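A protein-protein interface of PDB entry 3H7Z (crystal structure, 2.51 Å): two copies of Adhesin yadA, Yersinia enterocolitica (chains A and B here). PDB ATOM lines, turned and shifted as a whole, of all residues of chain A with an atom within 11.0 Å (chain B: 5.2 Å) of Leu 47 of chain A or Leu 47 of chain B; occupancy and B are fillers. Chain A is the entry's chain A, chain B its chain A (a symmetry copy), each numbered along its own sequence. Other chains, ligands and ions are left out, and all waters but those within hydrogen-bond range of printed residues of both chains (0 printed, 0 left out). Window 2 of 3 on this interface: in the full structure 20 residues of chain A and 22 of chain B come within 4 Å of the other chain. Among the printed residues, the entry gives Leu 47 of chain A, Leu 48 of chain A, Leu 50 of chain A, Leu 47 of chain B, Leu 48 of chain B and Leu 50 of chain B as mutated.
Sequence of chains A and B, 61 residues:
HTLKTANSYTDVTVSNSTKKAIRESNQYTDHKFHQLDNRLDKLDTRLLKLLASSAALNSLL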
ATOM      1  N   ARG A  39     -32.506   3.542 -14.809  1.00  0.00           N
ATOM      2  CA  ARG A  39     -31.843   3.804 -16.074  1.00  0.00           C
ATOM      3  C   ARG A  39     -30.698   4.793 -15.893  1.00  0.00           C
ATOM      4  O   ARG A  39     -29.815   4.928 -16.757  1.00  0.00           O
ATOM      5  CB  ARG A  39     -32.843   4.371 -17.064  1.00  0.00           C
ATOM      6  CG  ARG A  39     -32.977   3.573 -18.332  1.00  0.00           C
ATOM      7  CD  ARG A  39     -34.247   3.963 -19.084  1.00  0.00           C
ATOM      8  NE  ARG A  39     -34.116   5.283 -19.701  1.00  0.00           N
ATOM      9  CZ  ARG A  39     -34.921   5.765 -20.641  1.00  0.00           C
ATOM     10  NH1 ARG A  39     -35.944   5.044 -21.085  1.00  0.00           N
ATOM     11  NH2 ARG A  39     -34.699   6.971 -21.134  1.00  0.00           N
ATOM     12  N   LEU A  40     -30.718   5.495 -14.770  1.00  0.00           N
ATOM     13  CA  LEU A  40     -29.652   6.399 -14.459  1.00  0.00           C
ATOM     14  C   LEU A  40     -28.495   5.656 -13.821  1.00  0.00           C
ATOM     15  O   LEU A  40     -27.379   5.855 -14.248  1.00  0.00           O
ATOM     16  CB  LEU A  40     -30.149   7.522 -13.557  1.00  0.00           C
ATOM     17  CG  LEU A  40     -30.541   8.818 -14.259  1.00  0.00           C
ATOM     18  CD1 LEU A  40     -31.593   9.597 -13.471  1.00  0.00           C
ATOM     19  CD2 LEU A  40     -29.299   9.660 -14.480  1.00  0.00           C
ATOM     20  N   ASP A  41     -28.752   4.811 -12.814  1.00  0.00           N
ATOM     21  CA  ASP A  41     -27.711   4.043 -12.101  1.00  0.00           C
ATOM     22  C   ASP A  41     -26.909   3.195 -13.077  1.00  0.00           C
ATOM     23  O   ASP A  41     -25.777   2.811 -12.793  1.00  0.00           O
ATOM     24  CB  ASP A  41     -28.321   3.058 -11.093  1.00  0.00           C
ATOM     25  CG  ASP A  41     -29.094   3.724  -9.951  1.00  0.00           C
ATOM     26  OD1 ASP A  41     -28.619   4.735  -9.371  1.00  0.00           O
ATOM     27  OD2 ASP A  41     -30.172   3.171  -9.608  1.00  0.00           O
ATOM     28  N   LYS A  42     -27.539   2.871 -14.201  1.00  0.00           N
ATOM     29  CA  LYS A  42     -26.950   2.088 -15.265  1.00  0.00           C
ATOM     30  C   LYS A  42     -26.140   2.928 -16.240  1.00  0.00           C
ATOM     31  O   LYS A  42     -25.333   2.392 -16.985  1.00  0.00           O
ATOM     32  CB  LYS A  42     -28.040   1.366 -16.044  1.00  0.00           C
ATOM     33  CG  LYS A  42     -28.377  -0.025 -15.523  1.00  0.00           C
ATOM     34  CD  LYS A  42     -29.005  -0.829 -16.650  1.00  0.00           C
ATOM     35  CE  LYS A  42     -29.282  -2.259 -16.244  1.00  0.00           C
ATOM     36  NZ  LYS A  42     -29.926  -3.021 -17.372  1.00  0.00           N
ATOM     37  N   LEU A  43     -26.377   4.234 -16.254  1.00  0.00           N
ATOM     38  CA  LEU A  43     -25.591   5.169 -17.051  1.00  0.00           C
ATOM     39  C   LEU A  43     -24.362   5.652 -16.319  1.00  0.00           C
ATOM     40  O   LEU A  43     -23.412   6.085 -16.939  1.00  0.00           O
ATOM     41  CB  LEU A  43     -26.421   6.404 -17.354  1.00  0.00           C
ATOM     42  CG  LEU A  43     -27.149   6.586 -18.672  1.00  0.00           C
ATOM     43  CD1 LEU A  43     -27.334   8.076 -18.868  1.00  0.00           C
ATOM     44  CD2 LEU A  43     -26.362   5.991 -19.803  1.00  0.00           C
ATOM     45  N   ASP A  44     -24.468   5.649 -14.996  1.00  0.00           N
ATOM     46  CA  ASP A  44     -23.476   6.084 -14.023  1.00  0.00           C
ATOM     47  C   ASP A  44     -22.355   5.079 -13.834  1.00  0.00           C
ATOM     48  O   ASP A  44     -21.322   5.395 -13.265  1.00  0.00           O
ATOM     49  CB  ASP A  44     -24.164   6.156 -12.652  1.00  0.00           C
ATOM     50  CG  ASP A  44     -25.001   7.388 -12.464  1.00  0.00           C
ATOM     51  OD1 ASP A  44     -25.420   7.980 -13.473  1.00  0.00           O
ATOM     52  OD2 ASP A  44     -25.242   7.757 -11.288  1.00  0.00           O
ATOM     53  N   THR A  45     -22.636   3.842 -14.219  1.00  0.00           N
ATOM     54  CA  THR A  45     -21.765   2.718 -14.001  1.00  0.00           C
ATOM     55  C   THR A  45     -21.073   2.497 -15.297  1.00  0.00           C
ATOM     56  O   THR A  45     -19.947   2.090 -15.292  1.00  0.00           O
ATOM     57  CB  THR A  45     -22.546   1.433 -13.636  1.00  0.00           C
ATOM     58  OG1 THR A  45     -21.647   0.444 -13.125  1.00  0.00           O
ATOM     59  CG2 THR A  45     -23.274   0.844 -14.860  1.00  0.00           C
ATOM     60  N   ARG A  46     -21.775   2.769 -16.396  1.00  0.00           N
ATOM     61  CA  ARG A  46     -21.245   2.741 -17.748  1.00  0.00           C
ATOM     62  C   ARG A  46     -20.312   3.908 -17.941  1.00  0.00           C
ATOM     63  O   ARG A  46     -19.442   3.896 -18.796  1.00  0.00           O
ATOM     64  CB  ARG A  46     -22.384   2.861 -18.773  1.00  0.00           C
ATOM     65  CG  ARG A  46     -23.053   1.554 -19.208  1.00  0.00           C
ATOM     66  CD  ARG A  46     -23.693   1.701 -20.588  1.00  0.00           C
ATOM     67  NE  ARG A  46     -23.743   0.423 -21.308  1.00  0.00           N
ATOM     68  CZ  ARG A  46     -24.017   0.285 -22.606  1.00  0.00           C
ATOM     69  NH1 ARG A  46     -24.263   1.349 -23.372  1.00  0.00           N
ATOM     70  NH2 ARG A  46     -24.029  -0.925 -23.155  1.00  0.00           N
ATOM     71  N   LEU A  47     -20.515   4.940 -17.150  1.00  0.00           N
ATOM     72  CA  LEU A  47     -19.747   6.147 -17.267  1.00  0.00           C
ATOM     73  C   LEU A  47     -18.613   6.072 -16.298  1.00  0.00           C
ATOM     74  O   LEU A  47     -17.620   6.739 -16.487  1.00  0.00           O
ATOM     75  CB  LEU A  47     -20.608   7.338 -16.900  1.00  0.00           C
ATOM     76  CG  LEU A  47     -20.572   8.577 -17.784  1.00  0.00           C
ATOM     77  CD1 LEU A  47     -21.957   9.173 -17.752  1.00  0.00           C
ATOM     78  CD2 LEU A  47     -19.547   9.565 -17.290  1.00  0.00           C
ATOM     79  N   LEU A  48     -18.780   5.289 -15.240  1.00  0.00           N
ATOM     80  CA  LEU A  48     -17.748   5.108 -14.236  1.00  0.00           C
ATOM     81  C   LEU A  48     -16.550   4.434 -14.875  1.00  0.00           C
ATOM     82  O   LEU A  48     -15.409   4.742 -14.544  1.00  0.00           O
ATOM     83  CB  LEU A  48     -18.229   4.175 -13.135  1.00  0.00           C
ATOM     84  CG  LEU A  48     -18.341   4.571 -11.674  1.00  0.00           C
ATOM     85  CD1 LEU A  48     -17.651   3.473 -10.850  1.00  0.00           C
ATOM     86  CD2 LEU A  48     -17.763   5.939 -11.345  1.00  0.00           C
ATOM     87  N   LYS A  49     -16.857   3.470 -15.735  1.00  0.00           N
ATOM     88  CA  LYS A  49     -15.902   2.641 -16.405  1.00  0.00           C
ATOM     89  C   LYS A  49     -15.183   3.499 -17.408  1.00  0.00           C
ATOM     90  O   LYS A  49     -13.980   3.375 -17.565  1.00  0.00           O
ATOM     91  CB  LYS A  49     -16.609   1.479 -17.094  1.00  0.00           C
ATOM     92  CG  LYS A  49     -17.051   0.408 -16.145  1.00  0.00           C
ATOM     93  CD  LYS A  49     -17.919  -0.645 -16.816  1.00  0.00           C
ATOM     94  CE  LYS A  49     -18.298  -1.745 -15.806  1.00  0.00           C
ATOM     95  NZ  LYS A  49     -19.322  -2.757 -16.249  1.00  0.00           N
ATOM     96  N   LEU A  50     -15.916   4.402 -18.051  1.00  0.00           N
ATOM     97  CA  LEU A  50     -15.331   5.357 -18.981  1.00  0.00           C
ATOM     98  C   LEU A  50     -14.347   6.297 -18.326  1.00  0.00           C
ATOM     99  O   LEU A  50     -13.437   6.752 -18.977  1.00  0.00           O
ATOM    100  CB  LEU A  50     -16.405   6.176 -19.697  1.00  0.00           C
ATOM    101  CG  LEU A  50     -17.177   5.699 -20.934  1.00  0.00           C
ATOM    102  CD1 LEU A  50     -18.300   6.677 -21.237  1.00  0.00           C
ATOM    103  CD2 LEU A  50     -16.274   5.556 -22.149  1.00  0.00           C
ATOM    104  N   LEU A  51     -14.542   6.620 -17.058  1.00  0.00           N
ATOM    105  CA  LEU A  51     -13.633   7.518 -16.363  1.00  0.00           C
ATOM    106  C   LEU A  51     -12.407   6.744 -15.928  1.00  0.00           C
ATOM    107  O   LEU A  51     -11.281   7.260 -15.973  1.00  0.00           O
ATOM    108  CB  LEU A  51     -14.308   8.215 -15.181  1.00  0.00           C
ATOM    109  CG  LEU A  51     -14.967   9.563 -15.550  1.00  0.00           C
ATOM    110  CD1 LEU A  51     -16.436   9.615 -15.150  1.00  0.00           C
ATOM    111  CD2 LEU A  51     -14.236  10.788 -14.999  1.00  0.00           C
ATOM    112  N   ALA A  52     -12.636   5.492 -15.525  1.00  0.00           N
ATOM    113  CA  ALA A  52     -11.581   4.566 -15.158  1.00  0.00           C
ATOM    114  C   ALA A  52     -10.608   4.476 -16.322  1.00  0.00           C
ATOM    115  O   ALA A  52      -9.482   4.903 -16.190  1.00  0.00           O
ATOM    116  CB  ALA A  52     -12.150   3.214 -14.832  1.00  0.00           C
ATOM    117  N   SER A  53     -11.056   3.977 -17.472  1.00  0.00           N
ATOM    118  CA  SER A  53     -10.158   3.808 -18.588  1.00  0.00           C
ATOM    119  C   SER A  53      -9.467   5.061 -19.038  1.00  0.00           C
ATOM    120  O   SER A  53      -8.324   4.997 -19.435  1.00  0.00           O
ATOM    121  CB  SER A  53     -10.763   3.059 -19.777  1.00  0.00           C
ATOM    122  OG  SER A  53     -12.118   2.747 -19.597  1.00  0.00           O
ATOM    123  N   SER A  54     -10.121   6.204 -18.944  1.00  0.00           N
ATOM    124  CA  SER A  54      -9.504   7.427 -19.424  1.00  0.00           C
ATOM    125  C   SER A  54      -8.579   8.030 -18.367  1.00  0.00           C
ATOM    126  O   SER A  54      -7.830   8.963 -18.624  1.00  0.00           O
ATOM    127  CB  SER A  54     -10.557   8.425 -19.857  1.00  0.00           C
ATOM    128  OG  SER A  54     -10.521   9.534 -18.995  1.00  0.00           O
ATOM    129  N   ALA A  55      -8.628   7.499 -17.162  1.00  0.00           N
ATOM    130  CA  ALA A  55      -7.597   7.825 -16.195  1.00  0.00           C
ATOM    131  C   ALA A  55      -6.362   7.014 -16.566  1.00  0.00           C
ATOM    132  O   ALA A  55      -5.280   7.503 -16.444  1.00  0.00           O
ATOM    133  CB  ALA A  55      -8.047   7.472 -14.817  1.00  0.00           C
ATOM    134  N   LEU B  43     -28.477  11.276 -23.655  1.00  0.00           N
ATOM    135  CA  LEU B  43     -27.229  11.029 -22.940  1.00  0.00           C
ATOM    136  C   LEU B  43     -26.656   9.666 -23.245  1.00  0.00           C
ATOM    137  O   LEU B  43     -25.471   9.452 -23.083  1.00  0.00           O
ATOM    138  CB  LEU B  43     -27.483  11.062 -21.444  1.00  0.00           C
ATOM    139  CG  LEU B  43     -27.203  12.291 -20.602  1.00  0.00           C
ATOM    140  CD1 LEU B  43     -26.984  11.811 -19.182  1.00  0.00           C
ATOM    141  CD2 LEU B  43     -25.994  13.023 -21.111  1.00  0.00           C
ATOM    142  N   ASP B  44     -27.553   8.752 -23.589  1.00  0.00           N
ATOM    143  CA  ASP B  44     -27.319   7.350 -23.907  1.00  0.00           C
ATOM    144  C   ASP B  44     -26.732   7.149 -25.292  1.00  0.00           C
ATOM    145  O   ASP B  44     -26.236   6.081 -25.613  1.00  0.00           O
ATOM    146  CB  ASP B  44     -28.683   6.647 -23.960  1.00  0.00           C
ATOM    147  CG  ASP B  44     -29.246   6.325 -22.607  1.00  0.00           C
ATOM    148  OD1 ASP B  44     -28.852   6.982 -21.629  1.00  0.00           O
ATOM    149  OD2 ASP B  44     -30.097   5.405 -22.532  1.00  0.00           O
ATOM    150  N   THR B  45     -26.910   8.160 -26.132  1.00  0.00           N
ATOM    151  CA  THR B  45     -26.554   8.118 -27.525  1.00  0.00           C
ATOM    152  C   THR B  45     -25.258   8.836 -27.623  1.00  0.00           C
ATOM    153  O   THR B  45     -24.458   8.481 -28.441  1.00  0.00           O
ATOM    154  CB  THR B  45     -27.588   8.845 -28.417  1.00  0.00           C
ATOM    155  OG1 THR B  45     -27.369   8.509 -29.791  1.00  0.00           O
ATOM    156  CG2 THR B  45     -27.489  10.375 -28.268  1.00  0.00           C
ATOM    157  N   ARG B  46     -25.077   9.850 -26.778  1.00  0.00           N
ATOM    158  CA  ARG B  46     -23.840  10.594 -26.628  1.00  0.00           C
ATOM    159  C   ARG B  46     -22.814   9.724 -25.950  1.00  0.00           C
ATOM    160  O   ARG B  46     -21.618   9.933 -26.071  1.00  0.00           O
ATOM    161  CB  ARG B  46     -24.066  11.840 -25.755  1.00  0.00           C
ATOM    162  CG  ARG B  46     -24.524  13.109 -26.479  1.00  0.00           C
ATOM    163  CD  ARG B  46     -24.143  14.357 -25.685  1.00  0.00           C
ATOM    164  NE  ARG B  46     -23.943  15.521 -26.558  1.00  0.00           N
ATOM    165  CZ  ARG B  46     -23.376  16.669 -26.186  1.00  0.00           C
ATOM    166  NH1 ARG B  46     -22.922  16.839 -24.942  1.00  0.00           N
ATOM    167  NH2 ARG B  46     -23.241  17.657 -27.064  1.00  0.00           N
ATOM    168  N   LEU B  47     -23.292   8.749 -25.205  1.00  0.00           N
ATOM    169  CA  LEU B  47     -22.434   7.884 -24.448  1.00  0.00           C
ATOM    170  C   LEU B  47     -22.169   6.660 -25.263  1.00  0.00           C
ATOM    171  O   LEU B  47     -21.181   5.997 -25.043  1.00  0.00           O
ATOM    172  CB  LEU B  47     -23.133   7.463 -23.171  1.00  0.00           C
ATOM    173  CG  LEU B  47     -22.361   7.497 -21.860  1.00  0.00           C
ATOM    174  CD1 LEU B  47     -23.352   7.859 -20.783  1.00  0.00           C
ATOM    175  CD2 LEU B  47     -21.716   6.165 -21.575  1.00  0.00           C
ATOM    176  N   LEU B  48     -23.076   6.343 -26.178  1.00  0.00           N
ATOM    177  CA  LEU B  48     -22.928   5.195 -27.053  1.00  0.00           C
ATOM    178  C   LEU B  48     -21.720   5.405 -27.943  1.00  0.00           C
ATOM    179  O   LEU B  48     -20.995   4.462 -28.245  1.00  0.00           O
ATOM    180  CB  LEU B  48     -24.128   5.070 -27.980  1.00  0.00           C
ATOM    181  CG  LEU B  48     -25.052   3.866 -28.018  1.00  0.00           C
ATOM    182  CD1 LEU B  48     -25.205   3.456 -29.490  1.00  0.00           C
ATOM    183  CD2 LEU B  48     -24.589   2.690 -27.173  1.00  0.00           C
ATOM    184  N   LYS B  49     -21.581   6.645 -28.398  1.00  0.00           N
ATOM    185  CA  LYS B  49     -20.565   7.069 -29.312  1.00  0.00           C
ATOM    186  C   LYS B  49     -19.255   7.043 -28.576  1.00  0.00           C
ATOM    187  O   LYS B  49     -18.251   6.633 -29.134  1.00  0.00           O
ATOM    188  CB  LYS B  49     -20.872   8.473 -29.822  1.00  0.00           C
ATOM    189  CG  LYS B  49     -21.970   8.506 -30.840  1.00  0.00           C
ATOM    190  CD  LYS B  49     -22.395   9.923 -31.195  1.00  0.00           C
ATOM    191  CE  LYS B  49     -23.486   9.895 -32.282  1.00  0.00           C
ATOM    192  NZ  LYS B  49     -24.165  11.201 -32.603  1.00  0.00           N
ATOM    193  N   LEU B  50     -19.279   7.435 -27.308  1.00  0.00           N
ATOM    194  CA  LEU B  50     -18.101   7.375 -26.454  1.00  0.00           C
ATOM    195  C   LEU B  50     -17.595   5.967 -26.240  1.00  0.00           C
ATOM    196  O   LEU B  50     -16.419   5.783 -26.033  1.00  0.00           O
ATOM    197  CB  LEU B  50     -18.356   8.027 -25.094  1.00  0.00           C
ATOM    198  CG  LEU B  50     -18.264   9.535 -24.826  1.00  0.00           C
ATOM    199  CD1 LEU B  50     -18.785   9.831 -23.431  1.00  0.00           C
ATOM    200  CD2 LEU B  50     -16.842  10.053 -24.969  1.00  0.00           C
ATOM    201  N   LEU B  51     -18.475   4.979 -26.250  1.00  0.00           N
ATOM    202  CA  LEU B  51     -18.058   3.600 -26.053  1.00  0.00           C
ATOM    203  C   LEU B  51     -17.506   3.059 -27.355  1.00  0.00           C
ATOM    204  O   LEU B  51     -16.527   2.296 -27.361  1.00  0.00           O
ATOM    205  CB  LEU B  51     -19.196   2.729 -25.518  1.00  0.00           C
ATOM    206  CG  LEU B  51     -19.259   2.672 -23.975  1.00  0.00           C
ATOM    207  CD1 LEU B  51     -20.629   3.067 -23.441  1.00  0.00           C
ATOM    208  CD2 LEU B  51     -18.839   1.328 -23.381  1.00  0.00           C
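Among the printed residues, pairs that only touch across the chains: Leu 43 of chain A with Leu 43 of chain B (3.8 Å), Leu 43 of chain A with Asp 44 of chain B (3.2 Å), Leu 43 of chain A with Leu 47 of chain B (3.7 Å), Leu 47 of chain A with Leu 47 of chain B (3.6 Å), Leu 50 of chain A with Leu 47 of chain B (3.5 Å) and Leu 50 of chain A with Leu 50 of chain B (3.9 Å).
Leu 47 of chain A touches just one residue of chain B: Leu 47 (3.6 Å). Of chain A, only Leu 43, Leu 47 and Leu 50 come within 4 Å of Leu 47 of chain B. Leu 43 of chain B touches just one residue of chain A: Leu 43 (3.8 Å). No residue of chain A comes within 4 Å of Thr 45 of chain B. No residue of chain A comes within 4 Å of Leu 48 of chain B. Of chain A, only Leu 50 (3.9 Å) comes within 4 Å of Leu 50 of chain B. No residue of chain A comes within 4 Å of Leu 51 of chain B. Of the printed residues of chain B, Leu 50 of chain A touches Leu 47 and Leu 50. Printed residues of chain B within 4 Å of Leu 43 of chain A: Leu 43 (3.8 Å), Asp 44 (3.2 Å) and Leu 47 (3.7 Å). Printed residues of chain A within 4 Å of Asp 44 of chain B: Leu 43 (3.2 Å). The nearest printed residue of chain B that does not touch Leu 47 of chain A is Leu 43 of chain B (5.9 Å). The nearest printed residue of chain A that does not touch Asp 44 of chain B is Arg 39 of chain A (4.9 Å).
Of the 17 printed residues of chain A, 3 touch a printed residue of chain B. Of the 9 printed residues of chain B, 4 touch a printed residue of chain A. Printed residues of chain B that touch a printed residue of chain A: Leu 43, Asp 44, Leu 47 and Leu 50. Among the printed residues, 6 pairs touch across the chains. Among the printed residues, no Asp or Glu carboxylate lies within 4 Å of a Lys or Arg side-chain nitrogen of the other chain.
Leu 43 of chain A touches Asp 44 of chain B, but with the chains exchanged Asp 44 of chain A does not touch Leu 43 of chain B (7.1 Å). Leu 43 of chain A touches Leu 47 of chain B, but with the chains exchanged Leu 47 of chain A does not touch Leu 43 of chain B (5.9 Å). Leu 50 of chain A touches Leu 47 of chain B, but with the chains exchanged Leu 47 of chain A does not touch Leu 50 of chain B (6.1 Å). Leu 50 of chain B touches its own counterpart, Leu 50 of chain A. Positions printed for both chains: 43, 44, 45, 46, 47, 48, 49, 50 and 51. Of the 6 pairs that touch across the chains among the printed residues, 3 have their exchanged pair printed and touching as well.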
